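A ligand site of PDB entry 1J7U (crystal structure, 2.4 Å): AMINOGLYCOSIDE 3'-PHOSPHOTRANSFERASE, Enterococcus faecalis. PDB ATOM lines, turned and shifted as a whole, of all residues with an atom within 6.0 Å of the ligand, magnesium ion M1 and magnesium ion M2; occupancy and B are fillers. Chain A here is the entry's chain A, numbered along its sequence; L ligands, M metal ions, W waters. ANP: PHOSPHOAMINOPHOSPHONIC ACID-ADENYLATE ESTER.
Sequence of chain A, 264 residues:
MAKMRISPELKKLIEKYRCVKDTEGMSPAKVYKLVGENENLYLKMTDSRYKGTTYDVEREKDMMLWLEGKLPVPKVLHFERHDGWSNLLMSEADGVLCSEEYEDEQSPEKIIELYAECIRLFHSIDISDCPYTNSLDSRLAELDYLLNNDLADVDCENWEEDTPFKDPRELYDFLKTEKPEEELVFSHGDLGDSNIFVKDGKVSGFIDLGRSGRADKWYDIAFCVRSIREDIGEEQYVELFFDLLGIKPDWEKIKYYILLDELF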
ATOM      1  N   ASP A  22      15.435  13.728  25.044  1.00  0.00           N
ATOM      2  CA  ASP A  22      16.312  14.406  24.084  1.00  0.00           C
ATOM      3  C   ASP A  22      17.349  15.290  24.796  1.00  0.00           C
ATOM      4  O   ASP A  22      17.033  15.981  25.757  1.00  0.00           O
ATOM      5  CB  ASP A  22      15.470  15.244  23.118  1.00  0.00           C
ATOM      6  CG  ASP A  22      16.305  15.975  22.091  1.00  0.00           C
ATOM      7  OD1 ASP A  22      17.059  15.318  21.343  1.00  0.00           O
ATOM      8  OD2 ASP A  22      16.204  17.223  22.037  1.00  0.00           O
ATOM      9  N   GLU A  24      19.221  17.859  23.305  1.00  0.00           N
ATOM     10  CA  GLU A  24      19.227  19.251  22.818  1.00  0.00           C
ATOM     11  C   GLU A  24      18.449  20.178  23.755  1.00  0.00           C
ATOM     12  O   GLU A  24      19.020  21.114  24.324  1.00  0.00           O
ATOM     13  CB  GLU A  24      18.653  19.309  21.405  1.00  0.00           C
ATOM     14  N   GLY A  25      17.144  19.940  23.864  1.00  0.00           N
ATOM     15  CA  GLY A  25      16.272  20.723  24.731  1.00  0.00           C
ATOM     16  C   GLY A  25      16.426  22.231  24.776  1.00  0.00           C
ATOM     17  O   GLY A  25      16.174  22.842  25.816  1.00  0.00           O
ATOM     18  N   MET A  26      16.797  22.839  23.647  1.00  0.00           N
ATOM     19  CA  MET A  26      16.988  24.290  23.570  1.00  0.00           C
ATOM     20  C   MET A  26      15.681  25.062  23.400  1.00  0.00           C
ATOM     21  O   MET A  26      15.673  26.189  22.895  1.00  0.00           O
ATOM     22  CB  MET A  26      17.955  24.639  22.439  1.00  0.00           C
ATOM     23  N   SER A  27      14.577  24.470  23.834  1.00  0.00           N
ATOM     24  CA  SER A  27      13.270  25.101  23.748  1.00  0.00           C
ATOM     25  C   SER A  27      12.448  24.714  24.972  1.00  0.00           C
ATOM     26  O   SER A  27      12.911  23.935  25.818  1.00  0.00           O
ATOM     27  CB  SER A  27      12.557  24.655  22.457  1.00  0.00           C
ATOM     28  OG  SER A  27      11.808  23.466  22.642  1.00  0.00           O
ATOM     29  N   PRO A  28      11.239  25.289  25.123  1.00  0.00           N
ATOM     30  CA  PRO A  28      10.368  24.982  26.256  1.00  0.00           C
ATOM     31  C   PRO A  28       9.788  23.570  26.173  1.00  0.00           C
ATOM     32  O   PRO A  28       9.406  22.977  27.180  1.00  0.00           O
ATOM     33  CB  PRO A  28       9.263  26.027  26.123  1.00  0.00           C
ATOM     34  CG  PRO A  28       9.939  27.170  25.397  1.00  0.00           C
ATOM     35  CD  PRO A  28      10.723  26.446  24.366  1.00  0.00           C
ATOM     36  N   ALA A  29       9.745  23.023  24.957  1.00  0.00           N
ATOM     37  CA  ALA A  29       9.199  21.687  24.711  1.00  0.00           C
ATOM     38  C   ALA A  29      10.066  20.535  25.171  1.00  0.00           C
ATOM     39  O   ALA A  29      11.288  20.549  25.022  1.00  0.00           O
ATOM     40  CB  ALA A  29       8.863  21.522  23.231  1.00  0.00           C
ATOM     41  N   VAL A  31      11.139  16.805  24.599  1.00  0.00           N
ATOM     42  CA  VAL A  31      11.173  15.847  23.493  1.00  0.00           C
ATOM     43  C   VAL A  31      11.670  14.504  23.993  1.00  0.00           C
ATOM     44  O   VAL A  31      12.702  14.423  24.653  1.00  0.00           O
ATOM     45  CB  VAL A  31      12.096  16.322  22.350  1.00  0.00           C
ATOM     46  CG1 VAL A  31      12.117  15.296  21.231  1.00  0.00           C
ATOM     47  CG2 VAL A  31      11.623  17.666  21.817  1.00  0.00           C
ATOM     48  N   TYR A  42       8.314   9.370  18.651  1.00  0.00           N
ATOM     49  CA  TYR A  42       8.753  10.566  19.360  1.00  0.00           C
ATOM     50  C   TYR A  42       7.556  11.230  20.010  1.00  0.00           C
ATOM     51  O   TYR A  42       6.461  11.220  19.465  1.00  0.00           O
ATOM     52  CB  TYR A  42       9.460  11.528  18.404  1.00  0.00           C
ATOM     53  CG  TYR A  42      10.917  11.207  18.177  1.00  0.00           C
ATOM     54  CD1 TYR A  42      11.315  10.342  17.164  1.00  0.00           C
ATOM     55  CD2 TYR A  42      11.909  11.804  18.972  1.00  0.00           C
ATOM     56  CE1 TYR A  42      12.668  10.073  16.936  1.00  0.00           C
ATOM     57  CE2 TYR A  42      13.257  11.545  18.752  1.00  0.00           C
ATOM     58  CZ  TYR A  42      13.627  10.687  17.738  1.00  0.00           C
ATOM     59  OH  TYR A  42      14.976  10.462  17.503  1.00  0.00           O
ATOM     60  N   LYS A  44       6.559  14.831  21.821  1.00  0.00           N
ATOM     61  CA  LYS A  44       6.931  16.208  22.094  1.00  0.00           C
ATOM     62  C   LYS A  44       5.768  16.790  22.863  1.00  0.00           C
ATOM     63  O   LYS A  44       4.598  16.525  22.533  1.00  0.00           O
ATOM     64  CB  LYS A  44       7.140  16.956  20.787  1.00  0.00           C
ATOM     65  CG  LYS A  44       7.889  18.254  20.902  1.00  0.00           C
ATOM     66  CD  LYS A  44       8.088  18.872  19.529  1.00  0.00           C
ATOM     67  CE  LYS A  44       8.913  20.143  19.596  1.00  0.00           C
ATOM     68  NZ  LYS A  44       9.201  20.638  18.224  1.00  0.00           N
ATOM     69  N   GLU A  60       1.694  22.748  16.335  1.00  0.00           N
ATOM     70  CA  GLU A  60       2.622  21.948  15.550  1.00  0.00           C
ATOM     71  C   GLU A  60       1.899  20.739  14.941  1.00  0.00           C
ATOM     72  O   GLU A  60       2.201  20.333  13.811  1.00  0.00           O
ATOM     73  CB  GLU A  60       3.774  21.516  16.442  1.00  0.00           C
ATOM     74  CG  GLU A  60       4.859  20.694  15.761  1.00  0.00           C
ATOM     75  CD  GLU A  60       6.085  20.531  16.635  1.00  0.00           C
ATOM     76  OE1 GLU A  60       5.953  20.644  17.867  1.00  0.00           O
ATOM     77  OE2 GLU A  60       7.180  20.325  16.090  1.00  0.00           O
ATOM     78  N   PRO A  74       6.495  13.814   9.726  1.00  0.00           N
ATOM     79  CA  PRO A  74       6.173  12.659  10.570  1.00  0.00           C
ATOM     80  C   PRO A  74       4.667  12.446  10.599  1.00  0.00           C
ATOM     81  O   PRO A  74       3.899  13.385  10.386  1.00  0.00           O
ATOM     82  CB  PRO A  74       6.675  13.091  11.939  1.00  0.00           C
ATOM     83  CG  PRO A  74       7.753  14.060  11.625  1.00  0.00           C
ATOM     84  CD  PRO A  74       7.149  14.855  10.523  1.00  0.00           C
ATOM     85  N   MET A  90       4.368  11.019  17.640  1.00  0.00           N
ATOM     86  CA  MET A  90       4.587  10.949  16.200  1.00  0.00           C
ATOM     87  C   MET A  90       5.568   9.859  15.780  1.00  0.00           C
ATOM     88  O   MET A  90       6.252   9.255  16.613  1.00  0.00           O
ATOM     89  CB  MET A  90       5.081  12.315  15.697  1.00  0.00           C
ATOM     90  CG  MET A  90       6.472  12.720  16.245  1.00  0.00           C
ATOM     91  SD  MET A  90       7.053  14.405  15.827  1.00  0.00           S
ATOM     92  CE  MET A  90       6.960  15.164  17.441  1.00  0.00           C
ATOM     93  N   SER A  91       5.620   9.621  14.475  1.00  0.00           N
ATOM     94  CA  SER A  91       6.515   8.630  13.906  1.00  0.00           C
ATOM     95  C   SER A  91       7.888   9.249  13.689  1.00  0.00           C
ATOM     96  O   SER A  91       8.029  10.476  13.641  1.00  0.00           O
ATOM     97  CB  SER A  91       5.966   8.127  12.578  1.00  0.00           C
ATOM     98  OG  SER A  91       5.764   9.186  11.668  1.00  0.00           O
ATOM     99  N   GLU A  92       8.890   8.398  13.572  1.00  0.00           N
ATOM    100  CA  GLU A  92      10.256   8.853  13.355  1.00  0.00           C
ATOM    101  C   GLU A  92      10.402   9.339  11.910  1.00  0.00           C
ATOM    102  O   GLU A  92       9.910   8.707  10.976  1.00  0.00           O
ATOM    103  CB  GLU A  92      11.239   7.713  13.626  1.00  0.00           C
ATOM    104  CG  GLU A  92      12.693   8.112  13.544  1.00  0.00           C
ATOM    105  CD  GLU A  92      13.617   7.033  14.051  1.00  0.00           C
ATOM    106  OE1 GLU A  92      13.527   5.892  13.542  1.00  0.00           O
ATOM    107  OE2 GLU A  92      14.431   7.312  14.961  1.00  0.00           O
ATOM    108  N   ALA A  93      11.065  10.472  11.736  1.00  0.00           N
ATOM    109  CA  ALA A  93      11.278  11.036  10.412  1.00  0.00           C
ATOM    110  C   ALA A  93      12.123  10.074   9.584  1.00  0.00           C
ATOM    111  O   ALA A  93      12.954   9.341  10.120  1.00  0.00           O
ATOM    112  CB  ALA A  93      11.980  12.384  10.532  1.00  0.00           C
ATOM    113  N   LEU A  97      19.438  12.900   9.734  1.00  0.00           N
ATOM    114  CA  LEU A  97      19.463  14.287  10.171  1.00  0.00           C
ATOM    115  C   LEU A  97      20.604  15.002   9.437  1.00  0.00           C
ATOM    116  O   LEU A  97      21.709  14.460   9.332  1.00  0.00           O
ATOM    117  CB  LEU A  97      19.693  14.342  11.687  1.00  0.00           C
ATOM    118  CG  LEU A  97      19.377  15.619  12.468  1.00  0.00           C
ATOM    119  CD1 LEU A  97      17.917  15.995  12.309  1.00  0.00           C
ATOM    120  CD2 LEU A  97      19.707  15.391  13.945  1.00  0.00           C
ATOM    121  N   ASP A 190      11.596  27.494  11.282  1.00  0.00           N
ATOM    122  CA  ASP A 190      12.896  27.270  11.907  1.00  0.00           C
ATOM    123  C   ASP A 190      13.720  26.333  11.023  1.00  0.00           C
ATOM    124  O   ASP A 190      14.071  25.228  11.421  1.00  0.00           O
ATOM    125  CB  ASP A 190      12.724  26.682  13.310  1.00  0.00           C
ATOM    126  CG  ASP A 190      14.024  26.667  14.093  1.00  0.00           C
ATOM    127  OD1 ASP A 190      15.002  27.315  13.664  1.00  0.00           O
ATOM    128  OD2 ASP A 190      14.066  26.008  15.151  1.00  0.00           O
ATOM    129  N   SER A 194      19.058  20.836  12.006  1.00  0.00           N
ATOM    130  CA  SER A 194      18.560  19.957  13.061  1.00  0.00           C
ATOM    131  C   SER A 194      17.091  19.590  12.880  1.00  0.00           C
ATOM    132  O   SER A 194      16.536  18.773  13.623  1.00  0.00           O
ATOM    133  CB  SER A 194      18.752  20.624  14.412  1.00  0.00           C
ATOM    134  OG  SER A 194      20.094  21.032  14.567  1.00  0.00           O
ATOM    135  N   ASN A 195      16.436  20.217  11.896  1.00  0.00           N
ATOM    136  CA  ASN A 195      15.025  19.967  11.640  1.00  0.00           C
ATOM    137  C   ASN A 195      14.783  19.393  10.242  1.00  0.00           C
ATOM    138  O   ASN A 195      13.637  19.219   9.844  1.00  0.00           O
ATOM    139  CB  ASN A 195      14.211  21.259  11.800  1.00  0.00           C
ATOM    140  CG  ASN A 195      14.342  21.882  13.174  1.00  0.00           C
ATOM    141  OD1 ASN A 195      14.488  21.190  14.186  1.00  0.00           O
ATOM    142  ND2 ASN A 195      14.271  23.196  13.229  1.00  0.00           N
ATOM    143  N   PHE A 197      15.807  16.335   7.259  1.00  0.00           N
ATOM    144  CA  PHE A 197      16.322  14.990   7.047  1.00  0.00           C
ATOM    145  C   PHE A 197      16.557  14.750   5.558  1.00  0.00           C
ATOM    146  O   PHE A 197      15.763  15.178   4.728  1.00  0.00           O
ATOM    147  CB  PHE A 197      15.351  13.943   7.596  1.00  0.00           C
ATOM    148  CG  PHE A 197      15.200  13.976   9.101  1.00  0.00           C
ATOM    149  CD1 PHE A 197      14.355  14.909   9.701  1.00  0.00           C
ATOM    150  CD2 PHE A 197      15.911  13.092   9.902  1.00  0.00           C
ATOM    151  CE1 PHE A 197      14.230  14.960  11.082  1.00  0.00           C
ATOM    152  CE2 PHE A 197      15.784  13.141  11.297  1.00  0.00           C
ATOM    153  CZ  PHE A 197      14.941  14.076  11.883  1.00  0.00           C
ATOM    154  N   ILE A 207      10.713  18.432  10.556  1.00  0.00           N
ATOM    155  CA  ILE A 207      10.161  18.317  11.910  1.00  0.00           C
ATOM    156  C   ILE A 207      10.245  19.720  12.521  1.00  0.00           C
ATOM    157  O   ILE A 207      10.780  20.638  11.873  1.00  0.00           O
ATOM    158  CB  ILE A 207      10.944  17.318  12.799  1.00  0.00           C
ATOM    159  CG1 ILE A 207      12.419  17.729  12.909  1.00  0.00           C
ATOM    160  CG2 ILE A 207      10.787  15.903  12.274  1.00  0.00           C
ATOM    161  CD1 ILE A 207      13.208  16.924  13.919  1.00  0.00           C
ATOM    162  N   ASP A 208       9.737  19.871  13.746  1.00  0.00           N
ATOM    163  CA  ASP A 208       9.739  21.159  14.451  1.00  0.00           C
ATOM    164  C   ASP A 208       8.894  22.155  13.643  1.00  0.00           C
ATOM    165  O   ASP A 208       9.407  23.137  13.118  1.00  0.00           O
ATOM    166  CB  ASP A 208      11.179  21.650  14.608  1.00  0.00           C
ATOM    167  CG  ASP A 208      11.381  22.526  15.838  1.00  0.00           C
ATOM    168  OD1 ASP A 208      10.381  22.924  16.467  1.00  0.00           O
ATOM    169  OD2 ASP A 208      12.548  22.813  16.163  1.00  0.00           O
ATOM    170  N   ARG A 211       6.213  26.606  14.309  1.00  0.00           N
ATOM    171  CA  ARG A 211       6.330  27.920  13.726  1.00  0.00           C
ATOM    172  C   ARG A 211       5.961  27.932  12.229  1.00  0.00           C
ATOM    173  O   ARG A 211       6.161  28.934  11.557  1.00  0.00           O
ATOM    174  CB  ARG A 211       7.755  28.456  13.939  1.00  0.00           C
ATOM    175  CG  ARG A 211       7.885  29.953  13.957  1.00  0.00           C
ATOM    176  CD  ARG A 211       8.232  30.444  15.358  1.00  0.00           C
ATOM    177  NE  ARG A 211       9.532  29.975  15.796  1.00  0.00           N
ATOM    178  CZ  ARG A 211       9.834  29.658  17.060  1.00  0.00           C
ATOM    179  NH1 ARG A 211       8.916  29.756  18.028  1.00  0.00           N
ATOM    180  NH2 ARG A 211      11.041  29.218  17.343  1.00  0.00           N
HETATM  181  PG  ANP L   1      14.767  23.296  18.655  1.00  0.00           P
HETATM  182  O1G ANP L   1      15.270  23.114  17.273  1.00  0.00           O
HETATM  183  O2G ANP L   1      15.786  23.231  19.728  1.00  0.00           O
HETATM  184  O3G ANP L   1      13.706  24.324  18.833  1.00  0.00           O
HETATM  185  PB  ANP L   1      12.714  21.564  19.668  1.00  0.00           P
HETATM  186  O1B ANP L   1      13.056  21.741  21.078  1.00  0.00           O
HETATM  187  O2B ANP L   1      11.580  22.327  19.087  1.00  0.00           O
HETATM  188  N3B ANP L   1      13.934  21.797  18.865  1.00  0.00           N
HETATM  189  PA  ANP L   1      12.571  19.247  17.978  1.00  0.00           P
HETATM  190  O1A ANP L   1      11.213  18.971  17.478  1.00  0.00           O
HETATM  191  O2A ANP L   1      13.530  19.992  17.124  1.00  0.00           O
HETATM  192  O3A ANP L   1      12.451  19.995  19.408  1.00  0.00           O
HETATM  193  O5' ANP L   1      13.260  17.867  18.411  1.00  0.00           O
HETATM  194  C5' ANP L   1      14.560  17.866  19.009  1.00  0.00           C
HETATM  195  C4' ANP L   1      15.444  16.827  18.323  1.00  0.00           C
HETATM  196  O4' ANP L   1      14.931  15.499  18.542  1.00  0.00           O
HETATM  197  C3' ANP L   1      15.458  16.961  16.805  1.00  0.00           C
HETATM  198  O3' ANP L   1      16.581  17.749  16.413  1.00  0.00           O
HETATM  199  C2' ANP L   1      15.699  15.502  16.402  1.00  0.00           C
HETATM  200  O2' ANP L   1      17.069  15.176  16.670  1.00  0.00           O
HETATM  201  C1' ANP L   1      14.844  14.694  17.364  1.00  0.00           C
HETATM  202  N9  ANP L   1      13.468  14.441  16.873  1.00  0.00           N
HETATM  203  C8  ANP L   1      12.291  15.000  17.290  1.00  0.00           C
HETATM  204  N7  ANP L   1      11.233  14.573  16.655  1.00  0.00           N
HETATM  205  C5  ANP L   1      11.743  13.655  15.745  1.00  0.00           C
HETATM  206  C6  ANP L   1      11.133  12.828  14.759  1.00  0.00           C
HETATM  207  N6  ANP L   1       9.821  12.802  14.529  1.00  0.00           N
HETATM  208  N1  ANP L   1      11.942  12.030  14.034  1.00  0.00           N
HETATM  209  C2  ANP L   1      13.252  12.047  14.262  1.00  0.00           C
HETATM  210  N3  ANP L   1      13.933  12.773  15.151  1.00  0.00           N
HETATM  211  C4  ANP L   1      13.108  13.565  15.873  1.00  0.00           C
HETATM  212 MG    MG M   1      14.545  21.611  16.203  1.00  0.00          MG
HETATM  213 MG    MG M   2      12.017  23.956  17.925  1.00  0.00          MG
HETATM  214  O   HOH W   1      10.318  24.546  18.962  1.00  0.00           O
HETATM  215  O   HOH W   2      16.211  20.450  16.225  1.00  0.00           O
HETATM  216  O   HOH W   3       9.346  17.163  16.845  1.00  0.00           O
HETATM  217  O   HOH W   4      12.014  25.546  16.578  1.00  0.00           O
HETATM  218  O   HOH W   5      17.056  12.605  15.677  1.00  0.00           O
HETATM  219  O   HOH W   6      16.493  23.447  15.140  1.00  0.00           O
HETATM  220  O   HOH W   7      13.515  20.736  23.428  1.00  0.00           O
HETATM  221  O   HOH W   8      16.805  20.322  19.055  1.00  0.00           O
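The side-chain hydroxyl (OG) of Ser 27 sits at hydrogen-bond distance from an oxygen (O1B) of the ligand (2.6 Å). NZ of Lys 44 is in salt-bridge range of O1A of the ligand (2.7 Å). N1 of the ligand is in hydrogen-bond range of N of Ala 93 (2.9 Å). O3' of the ligand lies within hydrogen-bond range of O of Ser 194 (3.0 Å). A nitrogen (N6) of the ligand is in hydrogen-bond range of the backbone carbonyl oxygen (O) of Ser 91 (3.1 Å). OH of Tyr 42 lies close to N3 of the ligand (3.5 Å). N6 of the ligand lies within hydrogen-bond range of SD of Met 90.
The backbone carbonyl oxygen (O) of Asn 195 is in hydrogen-bond range of the backbone NH (N) of Ile 207 (3.1 Å). ND2 of Asn 195 lies within hydrogen-bond range of O of Asp 190 (2.7 Å). The side-chain carboxylate of Asp 208 sits close to the side-chain amino group of Lys 44 (3.1 Å). OE2 of Glu 60 sits close to N of Asp 208. The side-chain hydroxyl (OG) of Ser 27 sits at hydrogen-bond distance from the backbone NH (N) of Ala 29. NZ of Lys 44 lies within salt-bridge range of OE2 of Glu 60, at 3.0 Å. O of Val 31 is in hydrogen-bond range of N of Asp 22. OD2 of Asp 22 lies close to N of Glu 24 (3.3 Å).
Merely in contact with the ligand: Asp 22 (3.5 Å), Met 26 (3.7 Å), Val 31 (3.5 Å), Pro 74 (3.8 Å), Glu 92 (3.7 Å), Leu 97 (3.8 Å), Asp 190 (3.8 Å), Phe 197 (3.6 Å) and Ile 207 (3.7 Å). Hydrophobic or aromatic side chains within 4 Å of the ligand: Met 26, Val 31, Tyr 42, Pro 74, Met 90, Ala 93, Leu 97, Phe 197 and Ile 207. Within 4 Å of the ligand: Asp 22, Met 26, Ser 27, Val 31, Tyr 42, Lys 44, Pro 74, Met 90, Ser 91, Glu 92, Ala 93, Leu 97, Asp 190, Ser 194, Asn 195, Phe 197, Ile 207 and Asp 208. The nearest printed residue that does not touch the ligand is Glu 60 (4.5 Å).
Within 4 Å of magnesium ion M2: Asp 208.
Magnesium ion M1 is bound by an oxygen (O1G) of the ligand, 2.0 Å away. Water W2 binds magnesium ion M1 (2.0 Å). OD1 of Asn 195 is bound to magnesium ion M1 (2.1 Å). Magnesium ion M1 is bound by O2A of the ligand, 2.1 Å away. Magnesium ion M1 is bound by the side-chain carboxylate (OD2) of Asp 208, 2.3 Å away. Slightly farther from magnesium ion M1 lies N3B of the ligand (2.7 Å).
Magnesium ion M2 is bound by an oxygen (O3G) of the ligand, an oxygen (O2B) of the ligand, water W1, water W4, the side-chain carboxylate (OD2) of Asp 208 and the side-chain carboxylate (OD1) of Asp 208.
Water W2 lies within hydrogen-bond range of an oxygen (O3') of the ligand and the backbone carbonyl oxygen (O) of Ser 194. Water W7 lies within hydrogen-bond range of O1B of the ligand (2.6 Å), O of Ala 29 (2.7 Å) and OG of Ser 27 (3.3 Å). Water W3 bridges an oxygen (O1A) of the ligand (2.7 Å) and the side-chain sulfur of Met 90 (3.7 Å).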
